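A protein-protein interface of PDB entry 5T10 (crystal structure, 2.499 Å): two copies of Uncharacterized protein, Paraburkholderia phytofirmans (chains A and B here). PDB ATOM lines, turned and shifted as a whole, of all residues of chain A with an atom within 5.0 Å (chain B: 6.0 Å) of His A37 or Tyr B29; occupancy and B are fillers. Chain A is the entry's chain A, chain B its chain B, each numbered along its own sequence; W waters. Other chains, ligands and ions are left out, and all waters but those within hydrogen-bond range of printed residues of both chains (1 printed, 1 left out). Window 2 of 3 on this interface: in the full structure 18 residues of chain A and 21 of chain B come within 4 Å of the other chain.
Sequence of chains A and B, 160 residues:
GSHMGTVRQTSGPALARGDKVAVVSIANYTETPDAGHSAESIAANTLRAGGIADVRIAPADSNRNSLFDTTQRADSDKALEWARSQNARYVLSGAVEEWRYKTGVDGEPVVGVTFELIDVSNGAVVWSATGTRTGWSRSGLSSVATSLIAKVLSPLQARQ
The side-chain carboxylate of Asp A34 is in hydrogen-bond range of a ring nitrogen (ND1) of His A37 (3.2 Å). The side-chain hydroxyl (OG) of Ser A38 sits at hydrogen-bond distance from the backbone carbonyl oxygen (O) of Asp A34, 3.3 Å away. The backbone carbonyl oxygen of His A37 sits at hydrogen-bond distance from the side-chain hydroxyl of Ser A41 (3.4 Å). The side-chain amide oxygen of Asn B28 lies within hydrogen-bond range of the side-chain hydroxyl of Thr B30 (2.9 Å). The backbone NH (N) of Tyr B29 is in hydrogen-bond range of the backbone carbonyl oxygen (O) of Val B96 (3.0 Å).
Pro A33 touches Tyr B29. Pro A33 touches Glu B31. O of Asn B28 touches OD2 of Asp A34 (3.6 Å). Tyr B29 touches Asp A34 (CA to OD2, 3.6 Å). His A37 touches Tyr B29 (CB to CZ, 3.5 Å). OG of Ser A38 touches CB of Tyr B29 (3.3 Å). CG of Glu B97 touches OG of Ser A38 (3.6 Å). Ser A41 touches Tyr B29. Glu B97 touches Ser A41 (OE2 to CB, 3.9 Å).
Of the printed residues of chain B, Pro A33 touches Tyr B29 (3.9 Å) and Glu B31 (3.6 Å). Of the printed residues of chain B, Asp A34 touches Asn B28 and Tyr B29. Gly A36 touches none of the printed residues of chain B. His A37 touches one residue of chain B. Of the printed residues of chain B, Ser A38 touches Tyr B29 and Glu B97. Ala A39 touches none of the printed residues of chain B. Of the printed residues of chain B, Ser A41 touches Tyr B29 (3.7 Å) and Glu B97 (3.9 Å). Of the printed residues of chain A, Asn B28 touches Asp A34 (3.6 Å). The nearest printed residue of chain B that does not touch Pro A33 is Thr B30 (5.6 Å).
Of the 9 printed residues of chain B, 4 touch a printed residue of chain A. Printed residues of chain B that touch a printed residue of chain A: Asn B28, Tyr B29, Glu B31 and Glu B97. Printed residues of chain A that touch a printed residue of chain B: Pro A33, Asp A34, His A37, Ser A38 and Ser A41. Among the printed residues, 9 pairs touch across the chains. Among the printed residues, no Asp or Glu carboxylate lies within 4 Å of a Lys or Arg side-chain nitrogen of the other chain.
No position is printed for both chains.
Water W1 bridges the side-chain hydroxyl (OH) of Tyr B29 (3.1 Å) and the side-chain carboxylate (OE1) of Glu A40 (3.4 Å).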
ATOM      1  N   ILE A  26       2.219  -7.209  20.857  1.00  0.00           N
ATOM      2  CA  ILE A  26       1.909  -6.605  22.145  1.00  0.00           C
ATOM      3  C   ILE A  26       2.062  -5.075  22.070  1.00  0.00           C
ATOM      4  O   ILE A  26       3.173  -4.547  21.977  1.00  0.00           O
ATOM      5  CB  ILE A  26       2.808  -7.222  23.248  1.00  0.00           C
ATOM      6  CG1 ILE A  26       2.461  -8.709  23.411  1.00  0.00           C
ATOM      7  CG2 ILE A  26       2.657  -6.489  24.565  1.00  0.00           C
ATOM      8  CD1 ILE A  26       2.897  -9.322  24.734  1.00  0.00           C
ATOM      9  N   PRO A  33      10.472   3.453  23.552  1.00  0.00           N
ATOM     10  CA  PRO A  33      10.485   2.708  22.288  1.00  0.00           C
ATOM     11  C   PRO A  33      10.754   1.215  22.486  1.00  0.00           C
ATOM     12  O   PRO A  33      11.533   0.806  23.356  1.00  0.00           O
ATOM     13  CB  PRO A  33      11.630   3.359  21.512  1.00  0.00           C
ATOM     14  CG  PRO A  33      11.742   4.741  22.104  1.00  0.00           C
ATOM     15  CD  PRO A  33      11.453   4.555  23.556  1.00  0.00           C
ATOM     16  N   ASP A  34      10.064   0.415  21.685  1.00  0.00           N
ATOM     17  CA  ASP A  34      10.220  -1.022  21.696  1.00  0.00           C
ATOM     18  C   ASP A  34       9.758  -1.679  22.995  1.00  0.00           C
ATOM     19  O   ASP A  34      10.070  -2.840  23.225  1.00  0.00           O
ATOM     20  CB  ASP A  34      11.671  -1.404  21.394  1.00  0.00           C
ATOM     21  CG  ASP A  34      12.051  -1.135  19.959  1.00  0.00           C
ATOM     22  OD1 ASP A  34      11.198  -1.337  19.074  1.00  0.00           O
ATOM     23  OD2 ASP A  34      13.209  -0.721  19.714  1.00  0.00           O
ATOM     24  N   ALA A  35       9.027  -0.954  23.842  1.00  0.00           N
ATOM     25  CA  ALA A  35       8.520  -1.552  25.083  1.00  0.00           C
ATOM     26  C   ALA A  35       7.729  -2.847  24.828  1.00  0.00           C
ATOM     27  O   ALA A  35       7.888  -3.848  25.543  1.00  0.00           O
ATOM     28  CB  ALA A  35       7.657  -0.560  25.847  1.00  0.00           C
ATOM     29  N   GLY A  36       6.888  -2.814  23.798  1.00  0.00           N
ATOM     30  CA  GLY A  36       6.063  -3.951  23.444  1.00  0.00           C
ATOM     31  C   GLY A  36       6.867  -5.126  22.915  1.00  0.00           C
ATOM     32  O   GLY A  36       6.583  -6.275  23.254  1.00  0.00           O
ATOM     33  N   HIS A  37       7.860  -4.844  22.077  1.00  0.00           N
ATOM     34  CA  HIS A  37       8.711  -5.900  21.557  1.00  0.00           C
ATOM     35  C   HIS A  37       9.529  -6.536  22.678  1.00  0.00           C
ATOM     36  O   HIS A  37       9.765  -7.746  22.679  1.00  0.00           O
ATOM     37  CB  HIS A  37       9.610  -5.407  20.424  1.00  0.00           C
ATOM     38  CG  HIS A  37       8.853  -4.927  19.219  1.00  0.00           C
ATOM     39  ND1 HIS A  37       9.062  -3.680  18.660  1.00  0.00           N
ATOM     40  CD2 HIS A  37       7.898  -5.520  18.474  1.00  0.00           C
ATOM     41  CE1 HIS A  37       8.261  -3.531  17.619  1.00  0.00           C
ATOM     42  NE2 HIS A  37       7.550  -4.632  17.479  1.00  0.00           N
ATOM     43  N   SER A  38       9.919  -5.731  23.655  1.00  0.00           N
ATOM     44  CA  SER A  38      10.602  -6.265  24.817  1.00  0.00           C
ATOM     45  C   SER A  38       9.685  -7.143  25.623  1.00  0.00           C
ATOM     46  O   SER A  38      10.123  -8.147  26.177  1.00  0.00           O
ATOM     47  CB  SER A  38      11.155  -5.160  25.697  1.00  0.00           C
ATOM     48  OG  SER A  38      12.217  -4.523  25.029  1.00  0.00           O
ATOM     49  N   ALA A  39       8.410  -6.762  25.675  1.00  0.00           N
ATOM     50  CA  ALA A  39       7.385  -7.526  26.378  1.00  0.00           C
ATOM     51  C   ALA A  39       7.073  -8.819  25.640  1.00  0.00           C
ATOM     52  O   ALA A  39       6.861  -9.845  26.274  1.00  0.00           O
ATOM     53  CB  ALA A  39       6.109  -6.686  26.582  1.00  0.00           C
ATOM     54  N   GLU A  40       7.060  -8.771  24.306  1.00  0.00           N
ATOM     55  CA  GLU A  40       6.927  -9.998  23.508  1.00  0.00           C
ATOM     56  C   GLU A  40       8.051 -10.984  23.799  1.00  0.00           C
ATOM     57  O   GLU A  40       7.806 -12.166  24.057  1.00  0.00           O
ATOM     58  CB  GLU A  40       6.914  -9.690  22.012  1.00  0.00           C
ATOM     59  CG  GLU A  40       5.587  -9.228  21.492  1.00  0.00           C
ATOM     60  CD  GLU A  40       5.709  -8.410  20.232  1.00  0.00           C
ATOM     61  OE1 GLU A  40       6.815  -8.378  19.658  1.00  0.00           O
ATOM     62  OE2 GLU A  40       4.703  -7.782  19.826  1.00  0.00           O
ATOM     63  N   SER A  41       9.291 -10.505  23.753  1.00  0.00           N
ATOM     64  CA  SER A  41      10.423 -11.407  23.932  1.00  0.00           C
ATOM     65  C   SER A  41      10.414 -12.016  25.326  1.00  0.00           C
ATOM     66  O   SER A  41      10.694 -13.190  25.481  1.00  0.00           O
ATOM     67  CB  SER A  41      11.771 -10.712  23.653  1.00  0.00           C
ATOM     68  OG  SER A  41      11.898 -10.348  22.285  1.00  0.00           O
ATOM     69  N   ALA B  27      18.342  -8.488  18.350  1.00  0.00           N
ATOM     70  CA  ALA B  27      17.556  -7.280  18.247  1.00  0.00           C
ATOM     71  C   ALA B  27      17.996  -6.256  19.279  1.00  0.00           C
ATOM     72  O   ALA B  27      18.436  -6.608  20.377  1.00  0.00           O
ATOM     73  CB  ALA B  27      16.069  -7.596  18.418  1.00  0.00           C
ATOM     74  N   ASN B  28      17.865  -4.984  18.921  1.00  0.00           N
ATOM     75  CA  ASN B  28      18.197  -3.906  19.838  1.00  0.00           C
ATOM     76  C   ASN B  28      16.956  -3.138  20.249  1.00  0.00           C
ATOM     77  O   ASN B  28      16.438  -2.311  19.494  1.00  0.00           O
ATOM     78  CB  ASN B  28      19.218  -2.955  19.224  1.00  0.00           C
ATOM     79  CG  ASN B  28      19.687  -1.911  20.206  1.00  0.00           C
ATOM     80  OD1 ASN B  28      19.442  -2.018  21.412  1.00  0.00           O
ATOM     81  ND2 ASN B  28      20.381  -0.889  19.699  1.00  0.00           N
ATOM     82  N   TYR B  29      16.487  -3.400  21.459  1.00  0.00           N
ATOM     83  CA  TYR B  29      15.274  -2.736  21.934  1.00  0.00           C
ATOM     84  C   TYR B  29      15.593  -1.637  22.930  1.00  0.00           C
ATOM     85  O   TYR B  29      14.776  -1.302  23.766  1.00  0.00           O
ATOM     86  CB  TYR B  29      14.336  -3.756  22.563  1.00  0.00           C
ATOM     87  CG  TYR B  29      13.818  -4.769  21.576  1.00  0.00           C
ATOM     88  CD1 TYR B  29      13.723  -4.460  20.229  1.00  0.00           C
ATOM     89  CD2 TYR B  29      13.416  -6.035  21.995  1.00  0.00           C
ATOM     90  CE1 TYR B  29      13.236  -5.378  19.320  1.00  0.00           C
ATOM     91  CE2 TYR B  29      12.923  -6.958  21.100  1.00  0.00           C
ATOM     92  CZ  TYR B  29      12.834  -6.622  19.764  1.00  0.00           C
ATOM     93  OH  TYR B  29      12.353  -7.533  18.865  1.00  0.00           O
ATOM     94  N   THR B  30      16.804  -1.109  22.858  1.00  0.00           N
ATOM     95  CA  THR B  30      17.214  -0.044  23.750  1.00  0.00           C
ATOM     96  C   THR B  30      17.533   1.190  22.931  1.00  0.00           C
ATOM     97  O   THR B  30      17.413   1.192  21.696  1.00  0.00           O
ATOM     98  CB  THR B  30      18.449  -0.428  24.553  1.00  0.00           C
ATOM     99  OG1 THR B  30      19.615  -0.228  23.746  1.00  0.00           O
ATOM    100  CG2 THR B  30      18.367  -1.902  24.989  1.00  0.00           C
ATOM    101  N   GLU B  31      17.911   2.250  23.625  1.00  0.00           N
ATOM    102  CA  GLU B  31      18.346   3.460  22.953  1.00  0.00           C
ATOM    103  C   GLU B  31      19.861   3.564  23.007  1.00  0.00           C
ATOM    104  O   GLU B  31      20.427   4.633  22.801  1.00  0.00           O
ATOM    105  CB  GLU B  31      17.685   4.688  23.570  1.00  0.00           C
ATOM    106  CG  GLU B  31      16.192   4.743  23.296  1.00  0.00           C
ATOM    107  CD  GLU B  31      15.531   5.920  23.960  1.00  0.00           C
ATOM    108  OE1 GLU B  31      15.948   6.273  25.085  1.00  0.00           O
ATOM    109  OE2 GLU B  31      14.604   6.500  23.352  1.00  0.00           O
ATOM    110  N   ALA B  95      17.401 -10.811  21.949  1.00  0.00           N
ATOM    111  CA  ALA B  95      17.199  -9.378  21.927  1.00  0.00           C
ATOM    112  C   ALA B  95      17.770  -8.766  23.196  1.00  0.00           C
ATOM    113  O   ALA B  95      17.947  -9.441  24.211  1.00  0.00           O
ATOM    114  CB  ALA B  95      15.728  -9.044  21.786  1.00  0.00           C
ATOM    115  N   VAL B  96      18.057  -7.476  23.133  1.00  0.00           N
ATOM    116  CA  VAL B  96      18.490  -6.753  24.311  1.00  0.00           C
ATOM    117  C   VAL B  96      17.384  -5.819  24.737  1.00  0.00           C
ATOM    118  O   VAL B  96      16.940  -4.975  23.958  1.00  0.00           O
ATOM    119  CB  VAL B  96      19.783  -5.977  24.045  1.00  0.00           C
ATOM    120  CG1 VAL B  96      20.179  -5.176  25.280  1.00  0.00           C
ATOM    121  CG2 VAL B  96      20.884  -6.958  23.644  1.00  0.00           C
ATOM    122  N   GLU B  97      16.927  -5.988  25.972  1.00  0.00           N
ATOM    123  CA  GLU B  97      15.815  -5.192  26.482  1.00  0.00           C
ATOM    124  C   GLU B  97      16.306  -3.969  27.241  1.00  0.00           C
ATOM    125  O   GLU B  97      15.615  -2.970  27.328  1.00  0.00           O
ATOM    126  CB  GLU B  97      14.886  -6.033  27.364  1.00  0.00           C
ATOM    127  CG  GLU B  97      14.120  -7.114  26.616  1.00  0.00           C
ATOM    128  CD  GLU B  97      14.925  -8.402  26.459  1.00  0.00           C
ATOM    129  OE1 GLU B  97      15.670  -8.785  27.395  1.00  0.00           O
ATOM    130  OE2 GLU B  97      14.810  -9.035  25.388  1.00  0.00           O
ATOM    131  N   GLU B  98      17.509  -4.060  27.789  1.00  0.00           N
ATOM    132  CA  GLU B  98      18.111  -2.951  28.507  1.00  0.00           C
ATOM    133  C   GLU B  98      19.615  -3.080  28.445  1.00  0.00           C
ATOM    134  O   GLU B  98      20.179  -4.184  28.580  1.00  0.00           O
ATOM    135  CB  GLU B  98      17.647  -2.942  29.960  1.00  0.00           C
ATOM    136  CG  GLU B  98      18.110  -1.744  30.770  1.00  0.00           C
ATOM    137  CD  GLU B  98      17.210  -1.487  31.975  1.00  0.00           C
ATOM    138  OE1 GLU B  98      16.843  -2.464  32.669  1.00  0.00           O
ATOM    139  OE2 GLU B  98      16.847  -0.306  32.210  1.00  0.00           O
HETATM  140  O   HOH W   1       9.980  -9.529  19.141  1.00  0.00           O
